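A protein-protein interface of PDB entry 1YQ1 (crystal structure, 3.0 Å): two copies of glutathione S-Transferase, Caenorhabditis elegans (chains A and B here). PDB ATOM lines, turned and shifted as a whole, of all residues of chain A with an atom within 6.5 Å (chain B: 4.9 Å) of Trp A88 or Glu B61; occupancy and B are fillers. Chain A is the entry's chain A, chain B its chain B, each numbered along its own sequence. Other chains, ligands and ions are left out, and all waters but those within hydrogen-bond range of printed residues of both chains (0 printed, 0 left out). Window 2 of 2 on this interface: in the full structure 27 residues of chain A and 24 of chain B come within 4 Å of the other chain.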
ATOM      1  N   PRO A  83      -4.780 -29.158 -19.605  1.00  0.00           N
ATOM      2  CA  PRO A  83      -4.348 -27.812 -19.994  1.00  0.00           C
ATOM      3  C   PRO A  83      -4.947 -27.394 -21.327  1.00  0.00           C
ATOM      4  O   PRO A  83      -5.212 -26.215 -21.555  1.00  0.00           O
ATOM      5  CB  PRO A  83      -2.835 -27.946 -20.059  1.00  0.00           C
ATOM      6  CG  PRO A  83      -2.555 -28.929 -18.996  1.00  0.00           C
ATOM      7  CD  PRO A  83      -3.611 -29.983 -19.260  1.00  0.00           C
ATOM      8  N   GLU A  84      -5.164 -28.373 -22.201  1.00  0.00           N
ATOM      9  CA  GLU A  84      -5.733 -28.106 -23.511  1.00  0.00           C
ATOM     10  C   GLU A  84      -7.197 -27.779 -23.367  1.00  0.00           C
ATOM     11  O   GLU A  84      -7.712 -26.917 -24.081  1.00  0.00           O
ATOM     12  CB  GLU A  84      -5.558 -29.305 -24.445  1.00  0.00           C
ATOM     13  CG  GLU A  84      -4.112 -29.632 -24.732  1.00  0.00           C
ATOM     14  CD  GLU A  84      -3.422 -30.282 -23.540  1.00  0.00           C
ATOM     15  OE1 GLU A  84      -4.021 -31.212 -22.935  1.00  0.00           O
ATOM     16  OE2 GLU A  84      -2.280 -29.868 -23.216  1.00  0.00           O
ATOM     17  N   GLU A  85      -7.869 -28.458 -22.441  1.00  0.00           N
ATOM     18  CA  GLU A  85      -9.287 -28.212 -22.211  1.00  0.00           C
ATOM     19  C   GLU A  85      -9.466 -26.808 -21.624  1.00  0.00           C
ATOM     20  O   GLU A  85     -10.330 -26.040 -22.050  1.00  0.00           O
ATOM     21  CB  GLU A  85      -9.857 -29.266 -21.267  1.00  0.00           C
ATOM     22  CG  GLU A  85     -11.290 -29.641 -21.617  1.00  0.00           C
ATOM     23  CD  GLU A  85     -11.855 -30.760 -20.763  1.00  0.00           C
ATOM     24  OE1 GLU A  85     -12.287 -30.499 -19.605  1.00  0.00           O
ATOM     25  OE2 GLU A  85     -11.861 -31.905 -21.271  1.00  0.00           O
ATOM     26  N   GLU A  86      -8.627 -26.474 -20.655  1.00  0.00           N
ATOM     27  CA  GLU A  86      -8.652 -25.161 -20.040  1.00  0.00           C
ATOM     28  C   GLU A  86      -8.498 -24.060 -21.086  1.00  0.00           C
ATOM     29  O   GLU A  86      -9.224 -23.067 -21.076  1.00  0.00           O
ATOM     30  CB  GLU A  86      -7.508 -25.043 -19.055  1.00  0.00           C
ATOM     31  CG  GLU A  86      -7.758 -25.685 -17.739  1.00  0.00           C
ATOM     32  CD  GLU A  86      -6.598 -25.477 -16.812  1.00  0.00           C
ATOM     33  OE1 GLU A  86      -6.577 -24.432 -16.121  1.00  0.00           O
ATOM     34  OE2 GLU A  86      -5.702 -26.350 -16.791  1.00  0.00           O
ATOM     35  N   ALA A  87      -7.524 -24.236 -21.973  1.00  0.00           N
ATOM     36  CA  ALA A  87      -7.251 -23.271 -23.027  1.00  0.00           C
ATOM     37  C   ALA A  87      -8.488 -23.053 -23.870  1.00  0.00           C
ATOM     38  O   ALA A  87      -8.706 -21.967 -24.397  1.00  0.00           O
ATOM     39  CB  ALA A  87      -6.114 -23.768 -23.900  1.00  0.00           C
ATOM     40  N   TRP A  88      -9.306 -24.087 -24.007  1.00  0.00           N
ATOM     41  CA  TRP A  88     -10.507 -23.929 -24.798  1.00  0.00           C
ATOM     42  C   TRP A  88     -11.562 -23.187 -24.024  1.00  0.00           C
ATOM     43  O   TRP A  88     -12.301 -22.389 -24.596  1.00  0.00           O
ATOM     44  CB  TRP A  88     -11.016 -25.279 -25.287  1.00  0.00           C
ATOM     45  CG  TRP A  88     -10.446 -25.583 -26.629  1.00  0.00           C
ATOM     46  CD1 TRP A  88      -9.182 -26.015 -26.904  1.00  0.00           C
ATOM     47  CD2 TRP A  88     -11.066 -25.327 -27.889  1.00  0.00           C
ATOM     48  NE1 TRP A  88      -8.974 -26.033 -28.259  1.00  0.00           N
ATOM     49  CE2 TRP A  88     -10.114 -25.614 -28.889  1.00  0.00           C
ATOM     50  CE3 TRP A  88     -12.334 -24.871 -28.270  1.00  0.00           C
ATOM     51  CZ2 TRP A  88     -10.387 -25.463 -30.248  1.00  0.00           C
ATOM     52  CZ3 TRP A  88     -12.608 -24.717 -29.621  1.00  0.00           C
ATOM     53  CH2 TRP A  88     -11.637 -25.011 -30.596  1.00  0.00           C
ATOM     54  N   VAL A  89     -11.632 -23.442 -22.722  1.00  0.00           N
ATOM     55  CA  VAL A  89     -12.582 -22.725 -21.882  1.00  0.00           C
ATOM     56  C   VAL A  89     -12.210 -21.242 -21.999  1.00  0.00           C
ATOM     57  O   VAL A  89     -13.079 -20.389 -22.182  1.00  0.00           O
ATOM     58  CB  VAL A  89     -12.493 -23.167 -20.399  1.00  0.00           C
ATOM     59  CG1 VAL A  89     -13.367 -22.275 -19.529  1.00  0.00           C
ATOM     60  CG2 VAL A  89     -12.952 -24.607 -20.260  1.00  0.00           C
ATOM     61  N   ASP A  90     -10.908 -20.951 -21.910  1.00  0.00           N
ATOM     62  CA  ASP A  90     -10.407 -19.588 -22.026  1.00  0.00           C
ATOM     63  C   ASP A  90     -10.806 -19.000 -23.359  1.00  0.00           C
ATOM     64  O   ASP A  90     -11.165 -17.829 -23.454  1.00  0.00           O
ATOM     65  CB  ASP A  90      -8.890 -19.552 -21.923  1.00  0.00           C
ATOM     66  CG  ASP A  90      -8.403 -19.733 -20.513  1.00  0.00           C
ATOM     67  OD1 ASP A  90      -9.138 -19.341 -19.591  1.00  0.00           O
ATOM     68  OD2 ASP A  90      -7.278 -20.245 -20.320  1.00  0.00           O
ATOM     69  N   ALA A  91     -10.740 -19.828 -24.391  1.00  0.00           N
ATOM     70  CA  ALA A  91     -11.083 -19.394 -25.736  1.00  0.00           C
ATOM     71  C   ALA A  91     -12.563 -19.146 -25.894  1.00  0.00           C
ATOM     72  O   ALA A  91     -12.959 -18.155 -26.476  1.00  0.00           O
ATOM     73  CB  ALA A  91     -10.629 -20.431 -26.744  1.00  0.00           C
ATOM     74  N   VAL A  92     -13.390 -20.049 -25.388  1.00  0.00           N
ATOM     75  CA  VAL A  92     -14.822 -19.862 -25.521  1.00  0.00           C
ATOM     76  C   VAL A  92     -15.177 -18.605 -24.737  1.00  0.00           C
ATOM     77  O   VAL A  92     -16.060 -17.853 -25.137  1.00  0.00           O
ATOM     78  CB  VAL A  92     -15.609 -21.113 -25.010  1.00  0.00           C
ATOM     79  CG1 VAL A  92     -15.381 -21.288 -23.551  1.00  0.00           C
ATOM     80  CG2 VAL A  92     -17.100 -20.994 -25.315  1.00  0.00           C
ATOM     81  N   HIS A  93     -14.464 -18.355 -23.639  1.00  0.00           N
ATOM     82  CA  HIS A  93     -14.714 -17.151 -22.837  1.00  0.00           C
ATOM     83  C   HIS A  93     -14.409 -15.873 -23.633  1.00  0.00           C
ATOM     84  O   HIS A  93     -15.192 -14.925 -23.629  1.00  0.00           O
ATOM     85  CB  HIS A  93     -13.883 -17.168 -21.550  1.00  0.00           C
ATOM     86  CG  HIS A  93     -14.112 -15.973 -20.674  1.00  0.00           C
ATOM     87  ND1 HIS A  93     -13.407 -14.797 -20.817  1.00  0.00           N
ATOM     88  CD2 HIS A  93     -14.989 -15.763 -19.663  1.00  0.00           C
ATOM     89  CE1 HIS A  93     -13.838 -13.917 -19.931  1.00  0.00           C
ATOM     90  NE2 HIS A  93     -14.799 -14.477 -19.220  1.00  0.00           N
ATOM     91  N   ILE A 137     -20.398 -21.267 -33.857  1.00  0.00           N
ATOM     92  CA  ILE A 137     -19.194 -21.777 -33.226  1.00  0.00           C
ATOM     93  C   ILE A 137     -19.624 -22.353 -31.880  1.00  0.00           C
ATOM     94  O   ILE A 137     -19.097 -23.361 -31.420  1.00  0.00           O
ATOM     95  CB  ILE A 137     -18.123 -20.634 -33.069  1.00  0.00           C
ATOM     96  CG1 ILE A 137     -16.963 -21.086 -32.180  1.00  0.00           C
ATOM     97  CG2 ILE A 137     -18.764 -19.379 -32.543  1.00  0.00           C
ATOM     98  CD1 ILE A 137     -17.271 -21.175 -30.709  1.00  0.00           C
ATOM     99  N   LEU A 141     -19.253 -26.685 -30.751  1.00  0.00           N
ATOM    100  CA  LEU A 141     -18.746 -27.275 -29.517  1.00  0.00           C
ATOM    101  C   LEU A 141     -19.868 -28.098 -28.915  1.00  0.00           C
ATOM    102  O   LEU A 141     -19.692 -29.253 -28.556  1.00  0.00           O
ATOM    103  CB  LEU A 141     -18.346 -26.169 -28.542  1.00  0.00           C
ATOM    104  CG  LEU A 141     -17.414 -25.139 -29.168  1.00  0.00           C
ATOM    105  CD1 LEU A 141     -17.264 -23.936 -28.264  1.00  0.00           C
ATOM    106  CD2 LEU A 141     -16.078 -25.795 -29.433  1.00  0.00           C
ATOM    107  N   LYS A 144     -20.002 -31.474 -30.748  1.00  0.00           N
ATOM    108  CA  LYS A 144     -18.786 -32.214 -30.432  1.00  0.00           C
ATOM    109  C   LYS A 144     -18.779 -32.590 -28.950  1.00  0.00           C
ATOM    110  O   LYS A 144     -17.872 -33.271 -28.479  1.00  0.00           O
ATOM    111  CB  LYS A 144     -17.564 -31.341 -30.748  1.00  0.00           C
ATOM    112  CG  LYS A 144     -17.489 -30.855 -32.204  1.00  0.00           C
ATOM    113  CD  LYS A 144     -16.687 -29.542 -32.379  1.00  0.00           C
ATOM    114  CE  LYS A 144     -15.204 -29.683 -32.009  1.00  0.00           C
ATOM    115  NZ  LYS A 144     -14.471 -28.376 -32.075  1.00  0.00           N
ATOM    116  N   ILE A 151     -17.466 -27.435 -23.250  1.00  0.00           N
ATOM    117  CA  ILE A 151     -16.238 -28.176 -23.397  1.00  0.00           C
ATOM    118  C   ILE A 151     -15.934 -28.922 -22.109  1.00  0.00           C
ATOM    119  O   ILE A 151     -16.323 -28.490 -21.019  1.00  0.00           O
ATOM    120  CB  ILE A 151     -15.039 -27.262 -23.796  1.00  0.00           C
ATOM    121  CG1 ILE A 151     -14.474 -26.552 -22.578  1.00  0.00           C
ATOM    122  CG2 ILE A 151     -15.461 -26.263 -24.855  1.00  0.00           C
ATOM    123  CD1 ILE A 151     -13.523 -27.411 -21.778  1.00  0.00           C
ATOM    124  N   ALA A 158     -16.901 -21.428 -18.272  1.00  0.00           N
ATOM    125  CA  ALA A 158     -17.229 -20.923 -19.602  1.00  0.00           C
ATOM    126  C   ALA A 158     -18.729 -21.006 -19.814  1.00  0.00           C
ATOM    127  O   ALA A 158     -19.327 -20.086 -20.361  1.00  0.00           O
ATOM    128  CB  ALA A 158     -16.531 -21.734 -20.655  1.00  0.00           C
ATOM    129  N   PRO B  48     -10.939 -22.868 -36.350  1.00  0.00           N
ATOM    130  CA  PRO B  48     -11.541 -23.292 -35.081  1.00  0.00           C
ATOM    131  C   PRO B  48     -12.735 -22.430 -34.638  1.00  0.00           C
ATOM    132  O   PRO B  48     -13.825 -22.954 -34.358  1.00  0.00           O
ATOM    133  CB  PRO B  48     -10.367 -23.224 -34.122  1.00  0.00           C
ATOM    134  CG  PRO B  48      -9.240 -23.699 -34.990  1.00  0.00           C
ATOM    135  CD  PRO B  48      -9.470 -22.955 -36.284  1.00  0.00           C
ATOM    136  N   MET B  49     -12.530 -21.114 -34.565  1.00  0.00           N
ATOM    137  CA  MET B  49     -13.618 -20.217 -34.192  1.00  0.00           C
ATOM    138  C   MET B  49     -13.841 -19.133 -35.239  1.00  0.00           C
ATOM    139  O   MET B  49     -14.192 -17.995 -34.927  1.00  0.00           O
ATOM    140  CB  MET B  49     -13.363 -19.609 -32.822  1.00  0.00           C
ATOM    141  CG  MET B  49     -13.847 -20.495 -31.701  1.00  0.00           C
ATOM    142  SD  MET B  49     -13.474 -19.746 -29.988  1.00  0.00           S
ATOM    143  CE  MET B  49     -13.447 -21.354 -28.927  1.00  0.00           C
ATOM    144  N   VAL B  54      -4.603 -18.853 -34.883  1.00  0.00           N
ATOM    145  CA  VAL B  54      -4.904 -20.190 -34.405  1.00  0.00           C
ATOM    146  C   VAL B  54      -3.589 -20.923 -34.208  1.00  0.00           C
ATOM    147  O   VAL B  54      -2.724 -20.923 -35.089  1.00  0.00           O
ATOM    148  CB  VAL B  54      -5.764 -20.991 -35.379  1.00  0.00           C
ATOM    149  CG1 VAL B  54      -6.053 -22.371 -34.791  1.00  0.00           C
ATOM    150  CG2 VAL B  54      -7.050 -20.263 -35.648  1.00  0.00           C
ATOM    151  N   LEU B  55      -3.442 -21.526 -33.033  1.00  0.00           N
ATOM    152  CA  LEU B  55      -2.243 -22.269 -32.694  1.00  0.00           C
ATOM    153  C   LEU B  55      -2.453 -23.735 -32.995  1.00  0.00           C
ATOM    154  O   LEU B  55      -3.552 -24.267 -32.845  1.00  0.00           O
ATOM    155  CB  LEU B  55      -1.917 -22.120 -31.216  1.00  0.00           C
ATOM    156  CG  LEU B  55      -0.702 -22.912 -30.743  1.00  0.00           C
ATOM    157  CD1 LEU B  55       0.566 -22.141 -31.078  1.00  0.00           C
ATOM    158  CD2 LEU B  55      -0.802 -23.133 -29.255  1.00  0.00           C
ATOM    159  N   ASN B  56      -1.378 -24.384 -33.410  1.00  0.00           N
ATOM    160  CA  ASN B  56      -1.423 -25.792 -33.739  1.00  0.00           C
ATOM    161  C   ASN B  56      -0.175 -26.396 -33.135  1.00  0.00           C
ATOM    162  O   ASN B  56       0.928 -25.930 -33.414  1.00  0.00           O
ATOM    163  CB  ASN B  56      -1.409 -25.950 -35.252  1.00  0.00           C
ATOM    164  CG  ASN B  56      -2.323 -27.050 -35.728  1.00  0.00           C
ATOM    165  OD1 ASN B  56      -1.983 -28.236 -35.651  1.00  0.00           O
ATOM    166  ND2 ASN B  56      -3.501 -26.667 -36.217  1.00  0.00           N
ATOM    167  N   GLY B  59      -1.107 -31.508 -33.750  1.00  0.00           N
ATOM    168  CA  GLY B  59      -2.529 -31.810 -33.766  1.00  0.00           C
ATOM    169  C   GLY B  59      -3.465 -30.860 -33.039  1.00  0.00           C
ATOM    170  O   GLY B  59      -4.424 -30.365 -33.630  1.00  0.00           O
ATOM    171  N   PHE B  60      -3.204 -30.616 -31.760  1.00  0.00           N
ATOM    172  CA  PHE B  60      -4.032 -29.724 -30.959  1.00  0.00           C
ATOM    173  C   PHE B  60      -4.240 -28.389 -31.658  1.00  0.00           C
ATOM    174  O   PHE B  60      -3.293 -27.798 -32.183  1.00  0.00           O
ATOM    175  CB  PHE B  60      -3.378 -29.470 -29.608  1.00  0.00           C
ATOM    176  CG  PHE B  60      -4.196 -28.618 -28.696  1.00  0.00           C
ATOM    177  CD1 PHE B  60      -5.580 -28.756 -28.651  1.00  0.00           C
ATOM    178  CD2 PHE B  60      -3.586 -27.679 -27.866  1.00  0.00           C
ATOM    179  CE1 PHE B  60      -6.345 -27.971 -27.791  1.00  0.00           C
ATOM    180  CE2 PHE B  60      -4.341 -26.883 -26.999  1.00  0.00           C
ATOM    181  CZ  PHE B  60      -5.723 -27.029 -26.962  1.00  0.00           C
ATOM    182  N   GLU B  61      -5.483 -27.917 -31.661  1.00  0.00           N
ATOM    183  CA  GLU B  61      -5.810 -26.644 -32.285  1.00  0.00           C
ATOM    184  C   GLU B  61      -6.386 -25.708 -31.244  1.00  0.00           C
ATOM    185  O   GLU B  61      -7.262 -26.093 -30.476  1.00  0.00           O
ATOM    186  CB  GLU B  61      -6.812 -26.842 -33.424  1.00  0.00           C
ATOM    187  CG  GLU B  61      -6.152 -26.945 -34.796  1.00  0.00           C
ATOM    188  CD  GLU B  61      -7.147 -27.041 -35.940  1.00  0.00           C
ATOM    189  OE1 GLU B  61      -8.327 -27.375 -35.692  1.00  0.00           O
ATOM    190  OE2 GLU B  61      -6.740 -26.786 -37.092  1.00  0.00           O
ATOM    191  N   LEU B  62      -5.891 -24.473 -31.231  1.00  0.00           N
ATOM    192  CA  LEU B  62      -6.334 -23.468 -30.271  1.00  0.00           C
ATOM    193  C   LEU B  62      -6.529 -22.088 -30.893  1.00  0.00           C
ATOM    194  O   LEU B  62      -5.574 -21.443 -31.317  1.00  0.00           O
ATOM    195  CB  LEU B  62      -5.310 -23.355 -29.154  1.00  0.00           C
ATOM    196  CG  LEU B  62      -5.640 -22.391 -28.033  1.00  0.00           C
ATOM    197  CD1 LEU B  62      -6.757 -22.976 -27.194  1.00  0.00           C
ATOM    198  CD2 LEU B  62      -4.409 -22.160 -27.201  1.00  0.00           C
ATOM    199  N   PRO B  63      -7.776 -21.614 -30.952  1.00  0.00           N
ATOM    200  CA  PRO B  63      -8.054 -20.300 -31.524  1.00  0.00           C
ATOM    201  C   PRO B  63      -8.126 -19.313 -30.360  1.00  0.00           C
ATOM    202  O   PRO B  63      -8.086 -19.727 -29.195  1.00  0.00           O
ATOM    203  CB  PRO B  63      -9.410 -20.507 -32.160  1.00  0.00           C
ATOM    204  CG  PRO B  63     -10.102 -21.308 -31.085  1.00  0.00           C
ATOM    205  CD  PRO B  63      -9.035 -22.321 -30.653  1.00  0.00           C
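The indole nitrogen of Trp A88 is in hydrogen-bond range of the backbone carbonyl oxygen of Glu B61, at 2.8 Å.
N of Leu B55 sits at hydrogen-bond distance from O of Leu B62, 2.7 Å away. OE2 of Glu B61 sits close to ND2 of Asn B56.
Glu A84 touches Phe B60. Ala A87 touches Leu B62. Met B49 touches Trp A88 (CE to CZ3, 3.5 Å). Trp A88 touches Phe B60. Leu B62 touches Trp A88. CD of Pro B63 touches CZ2 of Trp A88, 3.4 Å away. Met B49 touches Ala A91 (CE to CB, 3.7 Å). Ala A91 touches Pro B63. Val A92 touches Met B49. Ile A137 touches Met B49 (CG1 to CG, 3.2 Å).
Of chain B, only Met B49, Phe B60, Glu B61, Leu B62 and Pro B63 come within 4 Å of Trp A88. Of chain A, only Trp A88 (2.8 Å) comes within 4 Å of Glu B61. Printed residues of chain B within 4 Å of Val A92: Met B49. Of the printed residues of chain A, Leu B62 touches Ala A87 and Trp A88. Of the printed residues of chain B, Ala A87 touches Leu B62 (3.4 Å). Lys A144 touches none of the printed residues of chain B. The nearest printed residue of chain A that does not touch Glu B61 is Glu A84 (6.5 Å).
Hydrophobic or aromatic side chains of chain B within 4 Å of the printed part of chain A: Met B49, Phe B60, Leu B62 and Pro B63. Hydrophobic or aromatic side chains of chain A within 4 Å of the printed part of chain B: Ala A87, Trp A88, Ala A91 and Ile A137. Among the printed residues, 11 pairs touch across the chains. Among the printed residues, no Asp or Glu carboxylate lies within 4 Å of a Lys or Arg side-chain nitrogen of the other chain.
No position is printed for both chains. Of the 11 pairs that touch across the chains among the printed residues, none has its exchanged pair printed and touching as well.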
